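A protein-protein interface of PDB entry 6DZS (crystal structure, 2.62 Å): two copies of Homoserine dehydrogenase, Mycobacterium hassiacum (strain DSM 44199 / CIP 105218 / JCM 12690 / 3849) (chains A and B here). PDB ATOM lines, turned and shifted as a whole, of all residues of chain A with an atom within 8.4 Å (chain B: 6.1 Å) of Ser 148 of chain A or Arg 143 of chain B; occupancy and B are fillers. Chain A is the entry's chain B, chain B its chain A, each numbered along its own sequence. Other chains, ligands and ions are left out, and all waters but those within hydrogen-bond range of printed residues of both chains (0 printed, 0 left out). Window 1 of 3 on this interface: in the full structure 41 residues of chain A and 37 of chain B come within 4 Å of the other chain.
The side-chain carboxylate (OE1) of Glu 132 of chain B sits at hydrogen-bond distance from the backbone NH (N) of Arg 143 of chain B (3.0 Å).
The side-chain amide nitrogen of Gln 147 of chain B lies close to the guanidinium group of Arg 143 of chain B, 3.3 Å away.
The guanidinium group (NH1) of Arg 327 of chain A sits at hydrogen-bond distance from the side-chain sulfur (SD) of Met 324 of chain A, 3.6 Å away.
NH2 of Arg 143 of chain B lies within salt-bridge range of OD1 of Asp 321 of chain B, 2.6 Å away.
OG1 of Thr 146 of chain B is in hydrogen-bond range of O of Ile 142 of chain B, at 2.9 Å.
The backbone NH (N) of Ala 299 of chain A is in hydrogen-bond range of the side-chain carboxylate (OD2) of Asp 152 of chain A (2.8 Å).
CB of Pro 140 of chain A touches OG of Ser 148 of chain B, at 3.5 Å.
Arg 143 of chain A touches Ser 148 of chain B.
Gly 320 of chain B touches Gln 147 of chain A.
SD of Met 324 of chain B touches CG of Gln 147 of chain A (3.6 Å).
Ser 148 of chain A touches Arg 143 of chain B.
Ser 148 of chain A touches Ser 316 of chain B.
Gly 320 of chain B touches Ser 148 of chain A.
OG of Ser 316 of chain B touches CD2 of Leu 149 of chain A, at 3.9 Å.
Ala 299 of chain A touches Ser 316 of chain B (CB to OG, 3.3 Å).
CE of Met 324 of chain A touches OE1 of Gln 147 of chain B (3.7 Å).
Pro 140 of chain A touches Ser 148 of chain B, and with the chains exchanged Ser 148 of chain A touches Pro 140 of chain B.
Arg 143 of chain A touches Gln 147 of chain B, and with the chains exchanged Gln 147 of chain A touches Arg 143 of chain B.
Arg 143 of chain A touches Ser 148 of chain B, and with the chains exchanged Ser 148 of chain A touches Arg 143 of chain B.
Gln 147 of chain A touches its own counterpart, Gln 147 of chain B.
12 positions are printed for both chains.
Of the 17 pairs that touch across the chains among the printed residues, 9 have their exchanged pair printed and touching as well.
Hydrophobic or aromatic side chains of chain A that line the printed part of chain B: Pro 140, Leu 149, Ala 299 and Met 324.
Printed residues of chain B that touch a printed residue of chain A: Pro 140, Arg 143, Thr 146, Gln 147, Ser 148, Ser 316, Met 319, Gly 320 and Met 324.
Among the printed residues, 17 pairs touch across the chains.
Among the printed residues, no Asp or Glu carboxylate lies within 4 Å of a Lys or Arg side-chain nitrogen of the other chain.
OE1 of Gln 147 of chain B lies within hydrogen-bond range of NH1 of Arg 143 of chain A (3.1 Å).
The guanidinium group of Arg 143 of chain B lies close to the side-chain amide oxygen of Gln 147 of chain A (3.4 Å).
The side-chain amide oxygen of Gln 147 of chain B sits close to the side-chain amide oxygen of Gln 147 of chain A (3.2 Å).
OG of Ser 316 of chain B sits at hydrogen-bond distance from OD2 of Asp 152 of chain A, at 2.6 Å.
O of Thr 146 of chain B sits at hydrogen-bond distance from NH1 of Arg 327 of chain A (3.0 Å).
Of chain B, only Pro 140, Arg 143, Ser 316 and Gly 320 come within 4 Å of Ser 148 of chain A.
Of the printed residues of chain A, Arg 143 of chain B touches Gln 147 (3.4 Å) and Ser 148 (3.6 Å).
Of the printed residues of chain A, Gln 147 of chain B touches Arg 143, Gln 147 and Met 324.
Printed residues of chain B within 4 Å of Arg 327 of chain A: Thr 146.
Val 141 of chain B touches none of the printed residues of chain A.
Ala 317 of chain B touches none of the printed residues of chain A.
The nearest residue of chain B that does not touch Ser 148 of chain A is Glu 132 of chain B (4.2 Å).
The nearest printed residue of chain B that does not touch Leu 149 of chain A is Gly 320 of chain B (5.0 Å).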
ATOM      1  N   PRO A 140      -2.113 -10.215 -17.030  1.00  0.00           N
ATOM      2  CA  PRO A 140      -0.910 -10.891 -16.531  1.00  0.00           C
ATOM      3  C   PRO A 140      -0.474 -10.305 -15.200  1.00  0.00           C
ATOM      4  O   PRO A 140       0.013  -9.174 -15.158  1.00  0.00           O
ATOM      5  CB  PRO A 140       0.127 -10.633 -17.632  1.00  0.00           C
ATOM      6  CG  PRO A 140      -0.662 -10.202 -18.827  1.00  0.00           C
ATOM      7  CD  PRO A 140      -1.846  -9.482 -18.277  1.00  0.00           C
ATOM      8  N   VAL A 141      -0.658 -11.050 -14.107  1.00  0.00           N
ATOM      9  CA  VAL A 141      -0.353 -10.568 -12.768  1.00  0.00           C
ATOM     10  C   VAL A 141       0.631 -11.479 -12.047  1.00  0.00           C
ATOM     11  O   VAL A 141       1.540 -10.997 -11.362  1.00  0.00           O
ATOM     12  CB  VAL A 141      -1.645 -10.404 -11.933  1.00  0.00           C
ATOM     13  CG1 VAL A 141      -1.318 -10.081 -10.481  1.00  0.00           C
ATOM     14  CG2 VAL A 141      -2.520  -9.313 -12.516  1.00  0.00           C
ATOM     15  N   ILE A 142       0.475 -12.795 -12.186  1.00  0.00           N
ATOM     16  CA  ILE A 142       1.346 -13.717 -11.467  1.00  0.00           C
ATOM     17  C   ILE A 142       2.748 -13.702 -12.060  1.00  0.00           C
ATOM     18  O   ILE A 142       3.743 -13.716 -11.323  1.00  0.00           O
ATOM     19  CB  ILE A 142       0.740 -15.132 -11.468  1.00  0.00           C
ATOM     20  CG1 ILE A 142      -0.509 -15.148 -10.584  1.00  0.00           C
ATOM     21  CG2 ILE A 142       1.762 -16.160 -10.979  1.00  0.00           C
ATOM     22  CD1 ILE A 142      -1.295 -16.423 -10.655  1.00  0.00           C
ATOM     23  N   ARG A 143       2.863 -13.687 -13.388  1.00  0.00           N
ATOM     24  CA  ARG A 143       4.193 -13.679 -13.988  1.00  0.00           C
ATOM     25  C   ARG A 143       4.944 -12.403 -13.635  1.00  0.00           C
ATOM     26  O   ARG A 143       6.121 -12.489 -13.249  1.00  0.00           O
ATOM     27  CB  ARG A 143       4.092 -13.884 -15.503  1.00  0.00           C
ATOM     28  CG  ARG A 143       5.420 -14.220 -16.149  1.00  0.00           C
ATOM     29  CD  ARG A 143       5.243 -14.642 -17.593  1.00  0.00           C
ATOM     30  NE  ARG A 143       4.491 -15.888 -17.719  1.00  0.00           N
ATOM     31  CZ  ARG A 143       5.029 -17.105 -17.668  1.00  0.00           C
ATOM     32  NH1 ARG A 143       6.336 -17.260 -17.486  1.00  0.00           N
ATOM     33  NH2 ARG A 143       4.254 -18.172 -17.798  1.00  0.00           N
ATOM     34  N   PRO A 144       4.340 -11.212 -13.722  1.00  0.00           N
ATOM     35  CA  PRO A 144       5.039 -10.005 -13.242  1.00  0.00           C
ATOM     36  C   PRO A 144       5.520 -10.097 -11.805  1.00  0.00           C
ATOM     37  O   PRO A 144       6.641  -9.666 -11.508  1.00  0.00           O
ATOM     38  CB  PRO A 144       3.976  -8.910 -13.407  1.00  0.00           C
ATOM     39  CG  PRO A 144       3.126  -9.387 -14.526  1.00  0.00           C
ATOM     40  CD  PRO A 144       3.094 -10.886 -14.434  1.00  0.00           C
ATOM     41  N   LEU A 145       4.706 -10.642 -10.897  1.00  0.00           N
ATOM     42  CA  LEU A 145       5.106 -10.691  -9.495  1.00  0.00           C
ATOM     43  C   LEU A 145       6.162 -11.759  -9.239  1.00  0.00           C
ATOM     44  O   LEU A 145       6.938 -11.635  -8.287  1.00  0.00           O
ATOM     45  CB  LEU A 145       3.891 -10.941  -8.602  1.00  0.00           C
ATOM     46  CG  LEU A 145       2.898  -9.799  -8.386  1.00  0.00           C
ATOM     47  CD1 LEU A 145       1.626 -10.341  -7.756  1.00  0.00           C
ATOM     48  CD2 LEU A 145       3.493  -8.711  -7.509  1.00  0.00           C
ATOM     49  N   THR A 146       6.208 -12.810 -10.062  1.00  0.00           N
ATOM     50  CA  THR A 146       7.163 -13.891  -9.852  1.00  0.00           C
ATOM     51  C   THR A 146       8.466 -13.707 -10.612  1.00  0.00           C
ATOM     52  O   THR A 146       9.483 -14.277 -10.205  1.00  0.00           O
ATOM     53  CB  THR A 146       6.576 -15.242 -10.279  1.00  0.00           C
ATOM     54  OG1 THR A 146       6.120 -15.164 -11.636  1.00  0.00           O
ATOM     55  CG2 THR A 146       5.437 -15.644  -9.378  1.00  0.00           C
ATOM     56  N   GLN A 147       8.460 -12.954 -11.710  1.00  0.00           N
ATOM     57  CA  GLN A 147       9.644 -12.809 -12.546  1.00  0.00           C
ATOM     58  C   GLN A 147      10.076 -11.362 -12.707  1.00  0.00           C
ATOM     59  O   GLN A 147      11.238 -11.035 -12.438  1.00  0.00           O
ATOM     60  CB  GLN A 147       9.391 -13.441 -13.927  1.00  0.00           C
ATOM     61  CG  GLN A 147       9.085 -14.933 -13.880  1.00  0.00           C
ATOM     62  CD  GLN A 147       8.986 -15.554 -15.262  1.00  0.00           C
ATOM     63  OE1 GLN A 147       9.271 -14.906 -16.269  1.00  0.00           O
ATOM     64  NE2 GLN A 147       8.579 -16.816 -15.315  1.00  0.00           N
ATOM     65  N   SER A 148       9.174 -10.475 -13.134  1.00  0.00           N
ATOM     66  CA  SER A 148       9.571  -9.097 -13.400  1.00  0.00           C
ATOM     67  C   SER A 148       9.942  -8.348 -12.126  1.00  0.00           C
ATOM     68  O   SER A 148      10.826  -7.483 -12.153  1.00  0.00           O
ATOM     69  CB  SER A 148       8.447  -8.366 -14.135  1.00  0.00           C
ATOM     70  OG  SER A 148       8.420  -8.737 -15.501  1.00  0.00           O
ATOM     71  N   LEU A 149       9.287  -8.655 -11.012  1.00  0.00           N
ATOM     72  CA  LEU A 149       9.533  -7.978  -9.748  1.00  0.00           C
ATOM     73  C   LEU A 149      10.336  -8.834  -8.778  1.00  0.00           C
ATOM     74  O   LEU A 149      10.441  -8.483  -7.598  1.00  0.00           O
ATOM     75  CB  LEU A 149       8.201  -7.569  -9.114  1.00  0.00           C
ATOM     76  CG  LEU A 149       7.428  -6.475  -9.852  1.00  0.00           C
ATOM     77  CD1 LEU A 149       6.006  -6.385  -9.345  1.00  0.00           C
ATOM     78  CD2 LEU A 149       8.132  -5.138  -9.684  1.00  0.00           C
ATOM     79  N   ALA A 150      10.908  -9.944  -9.249  1.00  0.00           N
ATOM     80  CA  ALA A 150      11.641 -10.846  -8.365  1.00  0.00           C
ATOM     81  C   ALA A 150      12.874 -10.181  -7.766  1.00  0.00           C
ATOM     82  O   ALA A 150      13.343 -10.591  -6.698  1.00  0.00           O
ATOM     83  CB  ALA A 150      12.045 -12.105  -9.131  1.00  0.00           C
ATOM     84  N   GLY A 151      13.420  -9.174  -8.436  1.00  0.00           N
ATOM     85  CA  GLY A 151      14.567  -8.457  -7.928  1.00  0.00           C
ATOM     86  C   GLY A 151      14.216  -7.259  -7.082  1.00  0.00           C
ATOM     87  O   GLY A 151      15.102  -6.476  -6.724  1.00  0.00           O
ATOM     88  N   ASP A 152      12.945  -7.095  -6.750  1.00  0.00           N
ATOM     89  CA  ASP A 152      12.445  -5.947  -6.014  1.00  0.00           C
ATOM     90  C   ASP A 152      11.831  -6.435  -4.707  1.00  0.00           C
ATOM     91  O   ASP A 152      11.769  -7.636  -4.431  1.00  0.00           O
ATOM     92  CB  ASP A 152      11.429  -5.170  -6.860  1.00  0.00           C
ATOM     93  CG  ASP A 152      11.302  -3.707  -6.443  1.00  0.00           C
ATOM     94  OD1 ASP A 152      11.482  -3.406  -5.243  1.00  0.00           O
ATOM     95  OD2 ASP A 152      11.012  -2.857  -7.316  1.00  0.00           O
ATOM     96  N   VAL A 154       8.327  -6.062  -2.931  1.00  0.00           N
ATOM     97  CA  VAL A 154       6.927  -5.661  -2.976  1.00  0.00           C
ATOM     98  C   VAL A 154       6.422  -5.487  -1.552  1.00  0.00           C
ATOM     99  O   VAL A 154       6.745  -6.281  -0.659  1.00  0.00           O
ATOM    100  CB  VAL A 154       6.098  -6.704  -3.746  1.00  0.00           C
ATOM    101  CG1 VAL A 154       4.618  -6.336  -3.735  1.00  0.00           C
ATOM    102  CG2 VAL A 154       6.615  -6.838  -5.173  1.00  0.00           C
ATOM    103  N   ALA A 299      10.449  -0.126  -7.812  1.00  0.00           N
ATOM    104  CA  ALA A 299       9.547   0.139  -8.928  1.00  0.00           C
ATOM    105  C   ALA A 299       8.558   1.257  -8.619  1.00  0.00           C
ATOM    106  O   ALA A 299       8.102   1.946  -9.535  1.00  0.00           O
ATOM    107  CB  ALA A 299       8.785  -1.134  -9.304  1.00  0.00           C
ATOM    108  N   LEU A 302       2.649   0.423  -9.517  1.00  0.00           N
ATOM    109  CA  LEU A 302       2.228  -0.093 -10.811  1.00  0.00           C
ATOM    110  C   LEU A 302       0.742  -0.421 -10.751  1.00  0.00           C
ATOM    111  O   LEU A 302       0.207  -0.736  -9.685  1.00  0.00           O
ATOM    112  CB  LEU A 302       3.014  -1.354 -11.201  1.00  0.00           C
ATOM    113  CG  LEU A 302       4.537  -1.270 -11.253  1.00  0.00           C
ATOM    114  CD1 LEU A 302       5.123  -2.665 -11.325  1.00  0.00           C
ATOM    115  CD2 LEU A 302       4.999  -0.452 -12.438  1.00  0.00           C
ATOM    116  N   PHE A 304      -2.160  -2.739 -13.163  1.00  0.00           N
ATOM    117  CA  PHE A 304      -2.494  -3.621 -14.273  1.00  0.00           C
ATOM    118  C   PHE A 304      -4.008  -3.644 -14.433  1.00  0.00           C
ATOM    119  O   PHE A 304      -4.725  -3.940 -13.473  1.00  0.00           O
ATOM    120  CB  PHE A 304      -1.956  -5.031 -14.017  1.00  0.00           C
ATOM    121  CG  PHE A 304      -0.482  -5.076 -13.716  1.00  0.00           C
ATOM    122  CD1 PHE A 304      -0.012  -4.847 -12.432  1.00  0.00           C
ATOM    123  CD2 PHE A 304       0.433  -5.359 -14.717  1.00  0.00           C
ATOM    124  CE1 PHE A 304       1.347  -4.889 -12.154  1.00  0.00           C
ATOM    125  CE2 PHE A 304       1.791  -5.404 -14.442  1.00  0.00           C
ATOM    126  CZ  PHE A 304       2.246  -5.169 -13.159  1.00  0.00           C
ATOM    127  N   MET A 324       4.455 -21.293 -22.978  1.00  0.00           N
ATOM    128  CA  MET A 324       5.681 -21.328 -22.191  1.00  0.00           C
ATOM    129  C   MET A 324       6.028 -22.755 -21.780  1.00  0.00           C
ATOM    130  O   MET A 324       7.190 -23.167 -21.879  1.00  0.00           O
ATOM    131  CB  MET A 324       5.546 -20.412 -20.972  1.00  0.00           C
ATOM    132  CG  MET A 324       5.515 -18.919 -21.325  1.00  0.00           C
ATOM    133  SD  MET A 324       6.972 -18.366 -22.247  1.00  0.00           S
ATOM    134  CE  MET A 324       8.254 -18.647 -21.030  1.00  0.00           C
ATOM    135  N   ARG A 327       7.304 -24.372 -24.934  1.00  0.00           N
ATOM    136  CA  ARG A 327       8.653 -23.878 -25.191  1.00  0.00           C
ATOM    137  C   ARG A 327       9.661 -24.558 -24.273  1.00  0.00           C
ATOM    138  O   ARG A 327      10.696 -25.059 -24.729  1.00  0.00           O
ATOM    139  CB  ARG A 327       8.710 -22.361 -24.999  1.00  0.00           C
ATOM    140  CG  ARG A 327       8.331 -21.529 -26.217  1.00  0.00           C
ATOM    141  CD  ARG A 327       8.253 -20.052 -25.839  1.00  0.00           C
ATOM    142  NE  ARG A 327       8.036 -19.180 -26.990  1.00  0.00           N
ATOM    143  CZ  ARG A 327       7.637 -17.915 -26.903  1.00  0.00           C
ATOM    144  NH1 ARG A 327       7.393 -17.373 -25.715  1.00  0.00           N
ATOM    145  NH2 ARG A 327       7.468 -17.193 -28.004  1.00  0.00           N
ATOM    146  N   PRO A 336      10.344 -20.452 -12.883  1.00  0.00           N
ATOM    147  CA  PRO A 336      10.845 -20.081 -11.549  1.00  0.00           C
ATOM    148  C   PRO A 336      10.307 -21.013 -10.475  1.00  0.00           C
ATOM    149  O   PRO A 336       9.095 -21.170 -10.315  1.00  0.00           O
ATOM    150  CB  PRO A 336      10.333 -18.646 -11.364  1.00  0.00           C
ATOM    151  CG  PRO A 336      10.059 -18.147 -12.744  1.00  0.00           C
ATOM    152  CD  PRO A 336       9.626 -19.344 -13.537  1.00  0.00           C
ATOM    153  N   TYR B 130      18.547 -10.277 -21.808  1.00  0.00           N
ATOM    154  CA  TYR B 130      17.336  -9.631 -21.320  1.00  0.00           C
ATOM    155  C   TYR B 130      17.469  -8.115 -21.409  1.00  0.00           C
ATOM    156  O   TYR B 130      18.513  -7.552 -21.065  1.00  0.00           O
ATOM    157  CB  TYR B 130      17.052 -10.046 -19.875  1.00  0.00           C
ATOM    158  CG  TYR B 130      16.643 -11.495 -19.704  1.00  0.00           C
ATOM    159  CD1 TYR B 130      15.935 -12.162 -20.696  1.00  0.00           C
ATOM    160  CD2 TYR B 130      16.953 -12.192 -18.544  1.00  0.00           C
ATOM    161  CE1 TYR B 130      15.552 -13.482 -20.541  1.00  0.00           C
ATOM    162  CE2 TYR B 130      16.570 -13.516 -18.379  1.00  0.00           C
ATOM    163  CZ  TYR B 130      15.870 -14.153 -19.382  1.00  0.00           C
ATOM    164  OH  TYR B 130      15.487 -15.467 -19.232  1.00  0.00           O
ATOM    165  N   GLU B 132      14.423  -5.937 -20.609  1.00  0.00           N
ATOM    166  CA  GLU B 132      13.140  -5.402 -20.159  1.00  0.00           C
ATOM    167  C   GLU B 132      13.254  -3.928 -19.792  1.00  0.00           C
ATOM    168  O   GLU B 132      12.366  -3.127 -20.111  1.00  0.00           O
ATOM    169  CB  GLU B 132      12.626  -6.210 -18.964  1.00  0.00           C
ATOM    170  CG  GLU B 132      11.407  -5.609 -18.252  1.00  0.00           C
ATOM    171  CD  GLU B 132      10.135  -5.681 -19.074  1.00  0.00           C
ATOM    172  OE1 GLU B 132       9.452  -6.727 -19.015  1.00  0.00           O
ATOM    173  OE2 GLU B 132       9.822  -4.690 -19.774  1.00  0.00           O
ATOM    174  N   PRO B 140       6.413  -3.531 -16.408  1.00  0.00           N
ATOM    175  CA  PRO B 140       6.671  -4.759 -17.176  1.00  0.00           C
ATOM    176  C   PRO B 140       5.896  -4.777 -18.479  1.00  0.00           C
ATOM    177  O   PRO B 140       4.668  -4.891 -18.458  1.00  0.00           O
ATOM    178  CB  PRO B 140       6.201  -5.877 -16.236  1.00  0.00           C
ATOM    179  CG  PRO B 140       6.128  -5.247 -14.877  1.00  0.00           C
ATOM    180  CD  PRO B 140       5.763  -3.817 -15.119  1.00  0.00           C
ATOM    181  N   VAL B 141       6.586  -4.667 -19.611  1.00  0.00           N
ATOM    182  CA  VAL B 141       5.915  -4.633 -20.904  1.00  0.00           C
ATOM    183  C   VAL B 141       6.496  -5.702 -21.814  1.00  0.00           C
ATOM    184  O   VAL B 141       5.756  -6.406 -22.510  1.00  0.00           O
ATOM    185  CB  VAL B 141       6.027  -3.245 -21.558  1.00  0.00           C
ATOM    186  CG1 VAL B 141       5.436  -3.267 -22.961  1.00  0.00           C
ATOM    187  CG2 VAL B 141       5.318  -2.213 -20.708  1.00  0.00           C
ATOM    188  N   ILE B 142       7.822  -5.843 -21.812  1.00  0.00           N
ATOM    189  CA  ILE B 142       8.453  -6.779 -22.735  1.00  0.00           C
ATOM    190  C   ILE B 142       8.159  -8.216 -22.323  1.00  0.00           C
ATOM    191  O   ILE B 142       7.859  -9.064 -23.170  1.00  0.00           O
ATOM    192  CB  ILE B 142       9.964  -6.499 -22.832  1.00  0.00           C
ATOM    193  CG1 ILE B 142      10.178  -5.180 -23.582  1.00  0.00           C
ATOM    194  CG2 ILE B 142      10.686  -7.644 -23.536  1.00  0.00           C
ATOM    195  CD1 ILE B 142      11.610  -4.703 -23.643  1.00  0.00           C
ATOM    196  N   ARG B 143       8.228  -8.512 -21.029  1.00  0.00           N
ATOM    197  CA  ARG B 143       8.005  -9.885 -20.597  1.00  0.00           C
ATOM    198  C   ARG B 143       6.542 -10.264 -20.815  1.00  0.00           C
ATOM    199  O   ARG B 143       6.267 -11.380 -21.270  1.00  0.00           O
ATOM    200  CB  ARG B 143       8.417 -10.079 -19.138  1.00  0.00           C
ATOM    201  CG  ARG B 143       8.604 -11.541 -18.742  1.00  0.00           C
ATOM    202  CD  ARG B 143       9.261 -11.677 -17.369  1.00  0.00           C
ATOM    203  NE  ARG B 143      10.611 -11.121 -17.358  1.00  0.00           N
ATOM    204  CZ  ARG B 143      11.715 -11.812 -17.630  1.00  0.00           C
ATOM    205  NH1 ARG B 143      11.649 -13.106 -17.931  1.00  0.00           N
ATOM    206  NH2 ARG B 143      12.894 -11.201 -17.600  1.00  0.00           N
ATOM    207  N   PRO B 144       5.576  -9.385 -20.515  1.00  0.00           N
ATOM    208  CA  PRO B 144       4.179  -9.727 -20.842  1.00  0.00           C
ATOM    209  C   PRO B 144       3.930  -9.948 -22.326  1.00  0.00           C
ATOM    210  O   PRO B 144       3.119 -10.810 -22.688  1.00  0.00           O
ATOM    211  CB  PRO B 144       3.389  -8.521 -20.310  1.00  0.00           C
ATOM    212  CG  PRO B 144       4.225  -7.977 -19.222  1.00  0.00           C
ATOM    213  CD  PRO B 144       5.654  -8.205 -19.634  1.00  0.00           C
ATOM    214  N   LEU B 145       4.593  -9.186 -23.199  1.00  0.00           N
ATOM    215  CA  LEU B 145       4.336  -9.310 -24.630  1.00  0.00           C
ATOM    216  C   LEU B 145       5.036 -10.517 -25.245  1.00  0.00           C
ATOM    217  O   LEU B 145       4.565 -11.039 -26.262  1.00  0.00           O
ATOM    218  CB  LEU B 145       4.775  -8.042 -25.363  1.00  0.00           C
ATOM    219  CG  LEU B 145       3.835  -6.836 -25.346  1.00  0.00           C
ATOM    220  CD1 LEU B 145       4.548  -5.617 -25.891  1.00  0.00           C
ATOM    221  CD2 LEU B 145       2.584  -7.115 -26.164  1.00  0.00           C
ATOM    222  N   THR B 146       6.150 -10.966 -24.658  1.00  0.00           N
ATOM    223  CA  THR B 146       6.880 -12.117 -25.176  1.00  0.00           C
ATOM    224  C   THR B 146       6.454 -13.436 -24.549  1.00  0.00           C
ATOM    225  O   THR B 146       6.662 -14.489 -25.161  1.00  0.00           O
ATOM    226  CB  THR B 146       8.387 -11.955 -24.940  1.00  0.00           C
ATOM    227  OG1 THR B 146       8.646 -11.865 -23.534  1.00  0.00           O
ATOM    228  CG2 THR B 146       8.899 -10.713 -25.617  1.00  0.00           C
ATOM    229  N   GLN B 147       5.884 -13.407 -23.344  1.00  0.00           N
ATOM    230  CA  GLN B 147       5.558 -14.629 -22.617  1.00  0.00           C
ATOM    231  C   GLN B 147       4.072 -14.727 -22.303  1.00  0.00           C
ATOM    232  O   GLN B 147       3.411 -15.663 -22.767  1.00  0.00           O
ATOM    233  CB  GLN B 147       6.389 -14.705 -21.325  1.00  0.00           C
ATOM    234  CG  GLN B 147       7.902 -14.778 -21.545  1.00  0.00           C
ATOM    235  CD  GLN B 147       8.681 -15.000 -20.253  1.00  0.00           C
ATOM    236  OE1 GLN B 147       8.130 -15.453 -19.250  1.00  0.00           O
ATOM    237  NE2 GLN B 147       9.969 -14.678 -20.276  1.00  0.00           N
ATOM    238  N   SER B 148       3.520 -13.787 -21.534  1.00  0.00           N
ATOM    239  CA  SER B 148       2.137 -13.919 -21.088  1.00  0.00           C
ATOM    240  C   SER B 148       1.157 -13.886 -22.252  1.00  0.00           C
ATOM    241  O   SER B 148       0.120 -14.557 -22.206  1.00  0.00           O
ATOM    242  CB  SER B 148       1.806 -12.814 -20.084  1.00  0.00           C
ATOM    243  OG  SER B 148       2.329 -13.125 -18.805  1.00  0.00           O
ATOM    244  N   LEU B 149       1.465 -13.119 -23.298  1.00  0.00           N
ATOM    245  CA  LEU B 149       0.626 -13.020 -24.483  1.00  0.00           C
ATOM    246  C   LEU B 149       1.176 -13.831 -25.652  1.00  0.00           C
ATOM    247  O   LEU B 149       0.922 -13.498 -26.815  1.00  0.00           O
ATOM    248  CB  LEU B 149       0.472 -11.557 -24.892  1.00  0.00           C
ATOM    249  CG  LEU B 149      -0.247 -10.666 -23.883  1.00  0.00           C
ATOM    250  CD1 LEU B 149      -0.053  -9.212 -24.246  1.00  0.00           C
ATOM    251  CD2 LEU B 149      -1.720 -10.997 -23.838  1.00  0.00           C
ATOM    252  N   SER B 316      14.636  -1.585 -10.874  1.00  0.00           N
ATOM    253  CA  SER B 316      13.676  -2.641 -10.579  1.00  0.00           C
ATOM    254  C   SER B 316      13.585  -3.624 -11.738  1.00  0.00           C
ATOM    255  O   SER B 316      13.633  -4.844 -11.545  1.00  0.00           O
ATOM    256  CB  SER B 316      12.305  -2.029 -10.283  1.00  0.00           C
ATOM    257  OG  SER B 316      11.374  -3.028  -9.902  1.00  0.00           O
ATOM    258  N   ALA B 317      13.470  -3.097 -12.961  1.00  0.00           N
ATOM    259  CA  ALA B 317      13.350  -3.951 -14.138  1.00  0.00           C
ATOM    260  C   ALA B 317      14.649  -4.693 -14.421  1.00  0.00           C
ATOM    261  O   ALA B 317      14.629  -5.889 -14.738  1.00  0.00           O
ATOM    262  CB  ALA B 317      12.944  -3.113 -15.347  1.00  0.00           C
ATOM    263  N   MET B 319      16.890  -5.600 -12.267  1.00  0.00           N
ATOM    264  CA  MET B 319      17.088  -6.632 -11.255  1.00  0.00           C
ATOM    265  C   MET B 319      16.172  -7.826 -11.486  1.00  0.00           C
ATOM    266  O   MET B 319      16.560  -8.967 -11.205  1.00  0.00           O
ATOM    267  CB  MET B 319      16.863  -6.043  -9.864  1.00  0.00           C
ATOM    268  CG  MET B 319      17.990  -5.128  -9.401  1.00  0.00           C
ATOM    269  SD  MET B 319      19.616  -5.898  -9.536  1.00  0.00           S
ATOM    270  CE  MET B 319      19.377  -7.380  -8.558  1.00  0.00           C
ATOM    271  N   GLY B 320      14.957  -7.589 -11.975  1.00  0.00           N
ATOM    272  CA  GLY B 320      14.110  -8.701 -12.365  1.00  0.00           C
ATOM    273  C   GLY B 320      14.765  -9.551 -13.434  1.00  0.00           C
ATOM    274  O   GLY B 320      14.785 -10.781 -13.349  1.00  0.00           O
ATOM    275  N   ASP B 321      15.330  -8.896 -14.451  1.00  0.00           N
ATOM    276  CA  ASP B 321      16.066  -9.621 -15.480  1.00  0.00           C
ATOM    277  C   ASP B 321      17.279 -10.335 -14.893  1.00  0.00           C
ATOM    278  O   ASP B 321      17.594 -11.463 -15.289  1.00  0.00           O
ATOM    279  CB  ASP B 321      16.498  -8.660 -16.585  1.00  0.00           C
ATOM    280  CG  ASP B 321      15.372  -8.318 -17.535  1.00  0.00           C
ATOM    281  OD1 ASP B 321      14.316  -8.986 -17.478  1.00  0.00           O
ATOM    282  OD2 ASP B 321      15.555  -7.388 -18.349  1.00  0.00           O
ATOM    283  N   MET B 324      16.207 -13.476 -12.993  1.00  0.00           N
ATOM    284  CA  MET B 324      15.831 -14.522 -13.935  1.00  0.00           C
ATOM    285  C   MET B 324      17.062 -15.129 -14.595  1.00  0.00           C
ATOM    286  O   MET B 324      17.173 -16.355 -14.709  1.00  0.00           O
ATOM    287  CB  MET B 324      14.870 -13.962 -14.983  1.00  0.00           C
ATOM    288  CG  MET B 324      13.464 -13.693 -14.443  1.00  0.00           C
ATOM    289  SD  MET B 324      12.714 -15.153 -13.684  1.00  0.00           S
ATOM    290  CE  MET B 324      12.760 -16.301 -15.063  1.00  0.00           C
ATOM    291  N   PRO B 336      13.312 -17.314 -22.772  1.00  0.00           N
ATOM    292  CA  PRO B 336      12.693 -17.306 -24.106  1.00  0.00           C
ATOM    293  C   PRO B 336      13.725 -17.249 -25.221  1.00  0.00           C
ATOM    294  O   PRO B 336      14.927 -17.141 -24.960  1.00  0.00           O
ATOM    295  CB  PRO B 336      11.815 -16.046 -24.089  1.00  0.00           C
ATOM    296  CG  PRO B 336      11.660 -15.688 -22.653  1.00  0.00           C
ATOM    297  CD  PRO B 336      12.912 -16.142 -21.974  1.00  0.00           C
